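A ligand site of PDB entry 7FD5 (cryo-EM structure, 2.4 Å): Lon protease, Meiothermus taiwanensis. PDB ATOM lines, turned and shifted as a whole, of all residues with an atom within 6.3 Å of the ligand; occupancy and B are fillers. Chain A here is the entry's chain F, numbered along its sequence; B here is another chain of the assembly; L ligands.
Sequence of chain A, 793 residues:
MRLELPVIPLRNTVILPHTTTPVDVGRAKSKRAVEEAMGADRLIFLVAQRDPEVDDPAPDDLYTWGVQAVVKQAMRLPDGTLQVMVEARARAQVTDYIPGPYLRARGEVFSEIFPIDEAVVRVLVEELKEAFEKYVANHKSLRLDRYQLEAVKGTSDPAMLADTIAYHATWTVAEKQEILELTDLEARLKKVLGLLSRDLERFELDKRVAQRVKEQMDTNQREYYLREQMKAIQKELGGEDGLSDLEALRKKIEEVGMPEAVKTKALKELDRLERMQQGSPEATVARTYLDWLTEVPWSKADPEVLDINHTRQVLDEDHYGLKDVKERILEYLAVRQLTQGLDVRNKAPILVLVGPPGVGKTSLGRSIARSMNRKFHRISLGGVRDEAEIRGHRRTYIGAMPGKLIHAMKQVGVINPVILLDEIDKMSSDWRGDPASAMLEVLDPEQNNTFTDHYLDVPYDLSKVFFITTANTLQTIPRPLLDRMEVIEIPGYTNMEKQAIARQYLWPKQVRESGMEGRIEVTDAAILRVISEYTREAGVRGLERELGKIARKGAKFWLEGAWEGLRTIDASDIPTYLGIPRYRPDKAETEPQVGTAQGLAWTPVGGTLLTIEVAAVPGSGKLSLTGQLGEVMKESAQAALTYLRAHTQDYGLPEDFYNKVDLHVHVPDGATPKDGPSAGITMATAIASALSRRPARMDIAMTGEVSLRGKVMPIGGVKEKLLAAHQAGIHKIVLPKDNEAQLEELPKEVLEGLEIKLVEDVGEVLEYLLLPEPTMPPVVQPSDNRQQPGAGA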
ATOM      1  N   LEU A 600       0.688 -26.589  -0.601  1.00  0.00           N
ATOM      2  CA  LEU A 600      -0.263 -25.916   0.260  1.00  0.00           C
ATOM      3  C   LEU A 600      -1.609 -25.928  -0.433  1.00  0.00           C
ATOM      4  O   LEU A 600      -1.681 -25.787  -1.647  1.00  0.00           O
ATOM      5  CB  LEU A 600       0.161 -24.487   0.543  1.00  0.00           C
ATOM      6  CG  LEU A 600       1.499 -24.280   1.247  1.00  0.00           C
ATOM      7  CD1 LEU A 600       1.870 -22.850   1.249  1.00  0.00           C
ATOM      8  CD2 LEU A 600       1.390 -24.738   2.636  1.00  0.00           C
ATOM      9  N   ALA A 601      -2.673 -26.085   0.331  1.00  0.00           N
ATOM     10  CA  ALA A 601      -3.996 -26.182  -0.248  1.00  0.00           C
ATOM     11  C   ALA A 601      -4.955 -25.249   0.474  1.00  0.00           C
ATOM     12  O   ALA A 601      -4.705 -24.824   1.589  1.00  0.00           O
ATOM     13  CB  ALA A 601      -4.531 -27.596  -0.171  1.00  0.00           C
ATOM     14  N   TRP A 602      -6.066 -24.947  -0.180  1.00  0.00           N
ATOM     15  CA  TRP A 602      -7.050 -24.001   0.314  1.00  0.00           C
ATOM     16  C   TRP A 602      -8.345 -24.754   0.536  1.00  0.00           C
ATOM     17  O   TRP A 602      -8.804 -25.453  -0.361  1.00  0.00           O
ATOM     18  CB  TRP A 602      -7.300 -22.894  -0.695  1.00  0.00           C
ATOM     19  CG  TRP A 602      -8.194 -21.828  -0.231  1.00  0.00           C
ATOM     20  CD1 TRP A 602      -7.857 -20.739   0.487  1.00  0.00           C
ATOM     21  CD2 TRP A 602      -9.617 -21.794  -0.365  1.00  0.00           C
ATOM     22  NE1 TRP A 602      -8.966 -19.988   0.750  1.00  0.00           N
ATOM     23  CE2 TRP A 602     -10.062 -20.626   0.246  1.00  0.00           C
ATOM     24  CE3 TRP A 602     -10.550 -22.627  -0.972  1.00  0.00           C
ATOM     25  CZ2 TRP A 602     -11.390 -20.272   0.282  1.00  0.00           C
ATOM     26  CZ3 TRP A 602     -11.868 -22.284  -0.938  1.00  0.00           C
ATOM     27  CH2 TRP A 602     -12.279 -21.117  -0.313  1.00  0.00           C
ATOM     28  N   THR A 603      -8.941 -24.595   1.681  1.00  0.00           N
ATOM     29  CA  THR A 603     -10.293 -25.078   1.903  1.00  0.00           C
ATOM     30  C   THR A 603     -11.109 -23.861   2.279  1.00  0.00           C
ATOM     31  O   THR A 603     -10.531 -22.821   2.581  1.00  0.00           O
ATOM     32  CB  THR A 603     -10.312 -26.151   2.996  1.00  0.00           C
ATOM     33  OG1 THR A 603      -9.736 -25.621   4.188  1.00  0.00           O
ATOM     34  CG2 THR A 603      -9.564 -27.360   2.574  1.00  0.00           C
ATOM     35  N   THR A 608      -4.530 -26.230   4.305  1.00  0.00           N
ATOM     36  CA  THR A 608      -3.954 -27.500   4.724  1.00  0.00           C
ATOM     37  C   THR A 608      -2.613 -27.657   4.053  1.00  0.00           C
ATOM     38  O   THR A 608      -2.247 -26.886   3.182  1.00  0.00           O
ATOM     39  CB  THR A 608      -4.846 -28.688   4.368  1.00  0.00           C
ATOM     40  OG1 THR A 608      -5.061 -28.708   2.962  1.00  0.00           O
ATOM     41  CG2 THR A 608      -6.197 -28.638   5.043  1.00  0.00           C
ATOM     42  N   LEU A 610      -0.332 -30.425   1.753  1.00  0.00           N
ATOM     43  CA  LEU A 610      -0.450 -31.603   0.908  1.00  0.00           C
ATOM     44  C   LEU A 610       0.911 -31.958   0.365  1.00  0.00           C
ATOM     45  O   LEU A 610       1.691 -31.074   0.022  1.00  0.00           O
ATOM     46  CB  LEU A 610      -1.379 -31.387  -0.274  1.00  0.00           C
ATOM     47  CG  LEU A 610      -2.858 -31.280   0.004  1.00  0.00           C
ATOM     48  CD1 LEU A 610      -3.555 -31.038  -1.288  1.00  0.00           C
ATOM     49  CD2 LEU A 610      -3.354 -32.555   0.616  1.00  0.00           C
ATOM     50  N   ILE A 612       3.067 -34.117  -2.586  1.00  0.00           N
ATOM     51  CA  ILE A 612       3.033 -34.768  -3.881  1.00  0.00           C
ATOM     52  C   ILE A 612       4.052 -35.873  -3.835  1.00  0.00           C
ATOM     53  O   ILE A 612       5.154 -35.670  -3.324  1.00  0.00           O
ATOM     54  CB  ILE A 612       3.370 -33.763  -4.985  1.00  0.00           C
ATOM     55  CG1 ILE A 612       2.492 -32.535  -4.888  1.00  0.00           C
ATOM     56  CG2 ILE A 612       3.231 -34.361  -6.333  1.00  0.00           C
ATOM     57  CD1 ILE A 612       1.080 -32.757  -5.087  1.00  0.00           C
ATOM     58  N   MET A 633      -5.841 -30.124 -12.686  1.00  0.00           N
ATOM     59  CA  MET A 633      -4.626 -30.567 -12.020  1.00  0.00           C
ATOM     60  C   MET A 633      -3.870 -31.565 -12.878  1.00  0.00           C
ATOM     61  O   MET A 633      -2.632 -31.559 -12.889  1.00  0.00           O
ATOM     62  CB  MET A 633      -5.019 -31.145 -10.680  1.00  0.00           C
ATOM     63  CG  MET A 633      -3.905 -31.301  -9.733  1.00  0.00           C
ATOM     64  SD  MET A 633      -4.582 -31.651  -8.119  1.00  0.00           S
ATOM     65  CE  MET A 633      -3.093 -31.787  -7.201  1.00  0.00           C
ATOM     66  N   VAL A 667      -1.197 -38.145  -4.961  1.00  0.00           N
ATOM     67  CA  VAL A 667      -1.434 -37.089  -3.989  1.00  0.00           C
ATOM     68  C   VAL A 667      -2.309 -37.644  -2.881  1.00  0.00           C
ATOM     69  O   VAL A 667      -3.530 -37.661  -2.998  1.00  0.00           O
ATOM     70  CB  VAL A 667      -2.091 -35.858  -4.638  1.00  0.00           C
ATOM     71  CG1 VAL A 667      -2.166 -34.753  -3.652  1.00  0.00           C
ATOM     72  CG2 VAL A 667      -1.353 -35.406  -5.835  1.00  0.00           C
ATOM     73  N   THR A 672     -10.211 -38.073  -0.907  1.00  0.00           N
ATOM     74  CA  THR A 672     -10.845 -36.763  -1.034  1.00  0.00           C
ATOM     75  C   THR A 672     -10.535 -36.123  -2.378  1.00  0.00           C
ATOM     76  O   THR A 672      -9.396 -36.162  -2.815  1.00  0.00           O
ATOM     77  CB  THR A 672     -10.359 -35.837   0.074  1.00  0.00           C
ATOM     78  OG1 THR A 672      -8.948 -35.660  -0.067  1.00  0.00           O
ATOM     79  CG2 THR A 672     -10.614 -36.453   1.405  1.00  0.00           C
ATOM     80  N   PRO A 673     -11.558 -35.592  -3.084  1.00  0.00           N
ATOM     81  CA  PRO A 673     -11.304 -34.922  -4.320  1.00  0.00           C
ATOM     82  C   PRO A 673     -10.357 -33.728  -4.182  1.00  0.00           C
ATOM     83  O   PRO A 673     -10.503 -33.027  -3.252  1.00  0.00           O
ATOM     84  CB  PRO A 673     -12.698 -34.374  -4.615  1.00  0.00           C
ATOM     85  CG  PRO A 673     -13.602 -35.449  -4.157  1.00  0.00           C
ATOM     86  CD  PRO A 673     -13.008 -35.693  -2.801  1.00  0.00           C
ATOM     87  N   LYS A 674      -9.434 -33.553  -5.113  1.00  0.00           N
ATOM     88  CA  LYS A 674      -8.482 -32.417  -5.114  1.00  0.00           C
ATOM     89  C   LYS A 674      -8.488 -31.839  -6.510  1.00  0.00           C
ATOM     90  O   LYS A 674      -8.525 -32.615  -7.427  1.00  0.00           O
ATOM     91  CB  LYS A 674      -7.101 -32.961  -4.769  1.00  0.00           C
ATOM     92  CG  LYS A 674      -7.032 -33.738  -3.477  1.00  0.00           C
ATOM     93  CD  LYS A 674      -5.685 -34.297  -3.194  1.00  0.00           C
ATOM     94  CE  LYS A 674      -5.763 -35.352  -2.118  1.00  0.00           C
ATOM     95  NZ  LYS A 674      -6.588 -36.482  -2.579  1.00  0.00           N
ATOM     96  N   ASP A 675      -8.445 -30.523  -6.674  1.00  0.00           N
ATOM     97  CA  ASP A 675      -8.495 -29.865  -8.007  1.00  0.00           C
ATOM     98  C   ASP A 675      -7.780 -28.530  -7.957  1.00  0.00           C
ATOM     99  O   ASP A 675      -7.523 -28.082  -6.872  1.00  0.00           O
ATOM    100  CB  ASP A 675      -9.911 -29.562  -8.416  1.00  0.00           C
ATOM    101  CG  ASP A 675     -10.135 -29.627  -9.914  1.00  0.00           C
ATOM    102  OD1 ASP A 675      -9.138 -29.724 -10.645  1.00  0.00           O
ATOM    103  OD2 ASP A 675     -11.299 -29.585 -10.343  1.00  0.00           O
ATOM    104  N   GLY A 676      -7.443 -27.934  -9.102  1.00  0.00           N
ATOM    105  CA  GLY A 676      -6.872 -26.585  -9.135  1.00  0.00           C
ATOM    106  C   GLY A 676      -5.555 -26.476  -9.830  1.00  0.00           C
ATOM    107  O   GLY A 676      -4.849 -27.450  -9.898  1.00  0.00           O
ATOM    108  N   PRO A 677      -5.161 -25.287 -10.312  1.00  0.00           N
ATOM    109  CA  PRO A 677      -3.864 -25.160 -10.918  1.00  0.00           C
ATOM    110  C   PRO A 677      -2.758 -24.584 -10.044  1.00  0.00           C
ATOM    111  O   PRO A 677      -1.687 -24.484 -10.547  1.00  0.00           O
ATOM    112  CB  PRO A 677      -4.231 -24.069 -11.898  1.00  0.00           C
ATOM    113  CG  PRO A 677      -5.128 -23.146 -11.138  1.00  0.00           C
ATOM    114  CD  PRO A 677      -5.990 -24.093 -10.330  1.00  0.00           C
ATOM    115  N   SER A 678      -3.007 -24.312  -8.774  1.00  0.00           N
ATOM    116  CA  SER A 678      -2.059 -23.584  -7.956  1.00  0.00           C
ATOM    117  C   SER A 678      -0.873 -24.405  -7.564  1.00  0.00           C
ATOM    118  O   SER A 678       0.112 -23.869  -7.062  1.00  0.00           O
ATOM    119  CB  SER A 678      -2.705 -23.202  -6.674  1.00  0.00           C
ATOM    120  OG  SER A 678      -3.177 -24.408  -6.057  1.00  0.00           O
ATOM    121  N   ALA A 679      -0.857 -25.721  -7.820  1.00  0.00           N
ATOM    122  CA  ALA A 679       0.352 -26.467  -7.373  1.00  0.00           C
ATOM    123  C   ALA A 679       1.158 -27.052  -8.537  1.00  0.00           C
ATOM    124  O   ALA A 679       1.753 -28.138  -8.363  1.00  0.00           O
ATOM    125  CB  ALA A 679       0.002 -27.530  -6.366  1.00  0.00           C
ATOM    126  N   GLY A 680       1.238 -26.326  -9.665  1.00  0.00           N
ATOM    127  CA  GLY A 680       2.049 -26.796 -10.806  1.00  0.00           C
ATOM    128  C   GLY A 680       3.510 -26.922 -10.432  1.00  0.00           C
ATOM    129  O   GLY A 680       4.151 -27.895 -10.867  1.00  0.00           O
ATOM    130  N   THR A 682       4.743 -27.537  -7.427  1.00  0.00           N
ATOM    131  CA  THR A 682       4.926 -28.673  -6.473  1.00  0.00           C
ATOM    132  C   THR A 682       5.070 -29.977  -7.260  1.00  0.00           C
ATOM    133  O   THR A 682       5.565 -30.952  -6.672  1.00  0.00           O
ATOM    134  CB  THR A 682       3.798 -28.701  -5.439  1.00  0.00           C
ATOM    135  OG1 THR A 682       3.400 -27.358  -5.171  1.00  0.00           O
ATOM    136  CG2 THR A 682       4.216 -29.365  -4.143  1.00  0.00           C
ATOM    137  N   MET A 683       4.641 -29.995  -8.517  1.00  0.00           N
ATOM    138  CA  MET A 683       4.782 -31.160  -9.365  1.00  0.00           C
ATOM    139  C   MET A 683       6.051 -31.107 -10.170  1.00  0.00           C
ATOM    140  O   MET A 683       6.678 -32.145 -10.390  1.00  0.00           O
ATOM    141  CB  MET A 683       3.589 -31.297 -10.291  1.00  0.00           C
ATOM    142  CG  MET A 683       2.360 -31.694  -9.600  1.00  0.00           C
ATOM    143  SD  MET A 683       1.013 -31.765 -10.735  1.00  0.00           S
ATOM    144  CE  MET A 683      -0.304 -32.148  -9.634  1.00  0.00           C
ATOM    145  N   THR A 703       4.064 -22.938  -3.705  1.00  0.00           N
ATOM    146  CA  THR A 703       2.847 -22.888  -4.486  1.00  0.00           C
ATOM    147  C   THR A 703       3.095 -22.058  -5.722  1.00  0.00           C
ATOM    148  O   THR A 703       4.026 -21.252  -5.770  1.00  0.00           O
ATOM    149  CB  THR A 703       1.683 -22.332  -3.663  1.00  0.00           C
ATOM    150  OG1 THR A 703       0.535 -22.191  -4.483  1.00  0.00           O
ATOM    151  CG2 THR A 703       2.070 -21.047  -3.045  1.00  0.00           C
ATOM    152  N   ILE A 715      -1.430 -16.976  -8.130  1.00  0.00           N
ATOM    153  CA  ILE A 715      -2.400 -17.910  -7.579  1.00  0.00           C
ATOM    154  C   ILE A 715      -3.398 -17.186  -6.706  1.00  0.00           C
ATOM    155  O   ILE A 715      -3.328 -15.964  -6.540  1.00  0.00           O
ATOM    156  CB  ILE A 715      -1.715 -18.986  -6.742  1.00  0.00           C
ATOM    157  CG1 ILE A 715      -1.016 -18.291  -5.612  1.00  0.00           C
ATOM    158  CG2 ILE A 715      -0.738 -19.720  -7.541  1.00  0.00           C
ATOM    159  CD1 ILE A 715      -0.661 -19.145  -4.530  1.00  0.00           C
ATOM    160  N   GLY A 716      -4.313 -17.936  -6.107  1.00  0.00           N
ATOM    161  CA  GLY A 716      -5.287 -17.360  -5.211  1.00  0.00           C
ATOM    162  C   GLY A 716      -5.190 -17.924  -3.810  1.00  0.00           C
ATOM    163  O   GLY A 716      -4.579 -18.964  -3.602  1.00  0.00           O
ATOM    164  N   GLY A 717      -5.781 -17.229  -2.845  1.00  0.00           N
ATOM    165  CA  GLY A 717      -5.857 -17.700  -1.475  1.00  0.00           C
ATOM    166  C   GLY A 717      -4.533 -17.745  -0.753  1.00  0.00           C
ATOM    167  O   GLY A 717      -4.125 -18.803  -0.274  1.00  0.00           O
ATOM    168  N   LYS A 721      -3.169 -20.152   3.063  1.00  0.00           N
ATOM    169  CA  LYS A 721      -2.057 -21.068   2.846  1.00  0.00           C
ATOM    170  C   LYS A 721      -0.867 -20.702   3.697  1.00  0.00           C
ATOM    171  O   LYS A 721      -0.218 -21.590   4.263  1.00  0.00           O
ATOM    172  CB  LYS A 721      -1.682 -21.070   1.383  1.00  0.00           C
ATOM    173  CG  LYS A 721      -2.740 -21.630   0.506  1.00  0.00           C
ATOM    174  CD  LYS A 721      -2.317 -21.609  -0.911  1.00  0.00           C
ATOM    175  CE  LYS A 721      -3.415 -22.110  -1.785  1.00  0.00           C
ATOM    176  NZ  LYS A 721      -3.030 -22.038  -3.195  1.00  0.00           N
ATOM    177  N   ALA B 671      -7.216 -22.486 -15.626  1.00  0.00           N
ATOM    178  CA  ALA B 671      -8.497 -22.627 -14.945  1.00  0.00           C
ATOM    179  C   ALA B 671      -9.659 -22.078 -15.727  1.00  0.00           C
ATOM    180  O   ALA B 671     -10.807 -22.342 -15.359  1.00  0.00           O
ATOM    181  CB  ALA B 671      -8.440 -21.940 -13.589  1.00  0.00           C
HETATM  182  C1  LIG L   1      -8.354 -29.397  -1.516  1.00  0.00           C
HETATM  183  C2  LIG L   1      -8.426 -28.759  -0.280  1.00  0.00           C
HETATM  184  C3  LIG L   1      -8.374 -30.813   0.791  1.00  0.00           C
HETATM  185  C4  LIG L   1      -8.292 -31.470  -0.445  1.00  0.00           C
HETATM  186  C5  LIG L   1      -8.340 -28.619  -2.778  1.00  0.00           C
HETATM  187  C6  LIG L   1      -8.089 -26.419  -3.826  1.00  0.00           C
HETATM  188  C7  LIG L   1      -9.079 -25.269  -3.995  1.00  0.00           C
HETATM  189  O1  LIG L   1      -6.038 -26.221  -2.605  1.00  0.00           O
HETATM  190  C8  LIG L   1      -6.703 -25.920  -3.586  1.00  0.00           C
HETATM  191  N1  LIG L   1      -6.236 -25.305  -4.637  1.00  0.00           N
HETATM  192  C9  LIG L   1      -4.871 -25.370  -4.995  1.00  0.00           C
HETATM  193  C10 LIG L   1      -4.850 -26.607  -5.879  1.00  0.00           C
HETATM  194  C11 LIG L   1      -4.263 -27.794  -5.197  1.00  0.00           C
HETATM  195  C12 LIG L   1      -4.879 -28.392  -4.133  1.00  0.00           C
HETATM  196  C13 LIG L   1      -4.302 -29.511  -3.528  1.00  0.00           C
HETATM  197  C14 LIG L   1      -3.092 -30.036  -3.945  1.00  0.00           C
HETATM  198  C15 LIG L   1      -2.477 -29.428  -5.013  1.00  0.00           C
HETATM  199  C16 LIG L   1      -3.075 -28.320  -5.610  1.00  0.00           C
HETATM  200  B1  LIG L   1      -4.563 -24.097  -5.783  1.00  0.00           B
HETATM  201  O2  LIG L   1      -5.481 -23.958  -6.886  1.00  0.00           O
HETATM  202  O3  LIG L   1      -4.640 -22.890  -4.991  1.00  0.00           O
HETATM  203  C17 LIG L   1      -9.058 -24.712  -5.403  1.00  0.00           C
HETATM  204  C18 LIG L   1      -9.241 -25.587  -6.456  1.00  0.00           C
HETATM  205  C19 LIG L   1      -9.227 -25.102  -7.759  1.00  0.00           C
HETATM  206  C20 LIG L   1      -9.025 -23.749  -8.035  1.00  0.00           C
HETATM  207  C21 LIG L   1      -8.834 -22.875  -6.987  1.00  0.00           C
HETATM  208  C22 LIG L   1      -8.852 -23.347  -5.674  1.00  0.00           C
HETATM  209  N2  LIG L   1      -8.416 -27.282  -2.714  1.00  0.00           N
HETATM  210  O4  LIG L   1      -8.217 -29.235  -3.823  1.00  0.00           O
HETATM  211  N3  LIG L   1      -8.285 -30.742  -1.571  1.00  0.00           N
HETATM  212  N4  LIG L   1      -8.449 -29.476   0.855  1.00  0.00           N
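The backbone NH (N) of Ser 678 sits close to an oxygen (O2) of the ligand (3.1 Å). B1 of the ligand is covalently linked to OG of Ser 678, 1.4 Å away. NZ of Lys 721 is in hydrogen-bond range of O3 of the ligand (2.6 Å). N of Trp 602 lies within hydrogen-bond range of O1 of the ligand (2.7 Å). A nitrogen (N2) of the ligand is in hydrogen-bond range of the backbone carbonyl oxygen (O) of Trp 602, at 3.0 Å. The backbone NH (N) of Asp 675 is in hydrogen-bond range of an oxygen (O4) of the ligand.
The backbone carbonyl oxygen (O) of Ser 678 sits at hydrogen-bond distance from the side-chain hydroxyl (OG1) of Thr 703 (3.1 Å). The side-chain amino group (NZ) of Lys 721 is in hydrogen-bond range of the backbone carbonyl oxygen (O) of Gly 716. The backbone carbonyl oxygen (O) of Thr 608 sits at hydrogen-bond distance from the backbone NH (N) of Ala 601 (3.0 Å). NZ of Lys 674 is in hydrogen-bond range of O of Thr 672. The backbone carbonyl oxygen (O) of Val 667 sits at hydrogen-bond distance from the side-chain amino group (NZ) of Lys 674, 3.3 Å away.
CA of Ala 601 touches O1 of the ligand (3.1 Å). CG2 of Thr 603 touches N4 of the ligand, at 2.9 Å. Leu 610 touches the ligand. Met 633 touches the ligand. Pro 673 touches the ligand (O to N3, 3.6 Å). Lys 674 touches the ligand. Gly 676 touches the ligand. CD of Pro 677 touches O2 of the ligand (3.5 Å). CB of Ala 679 touches C16 of the ligand, 3.3 Å away. The nearest printed residue that does not touch the ligand is Thr 608 (4.1 Å).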
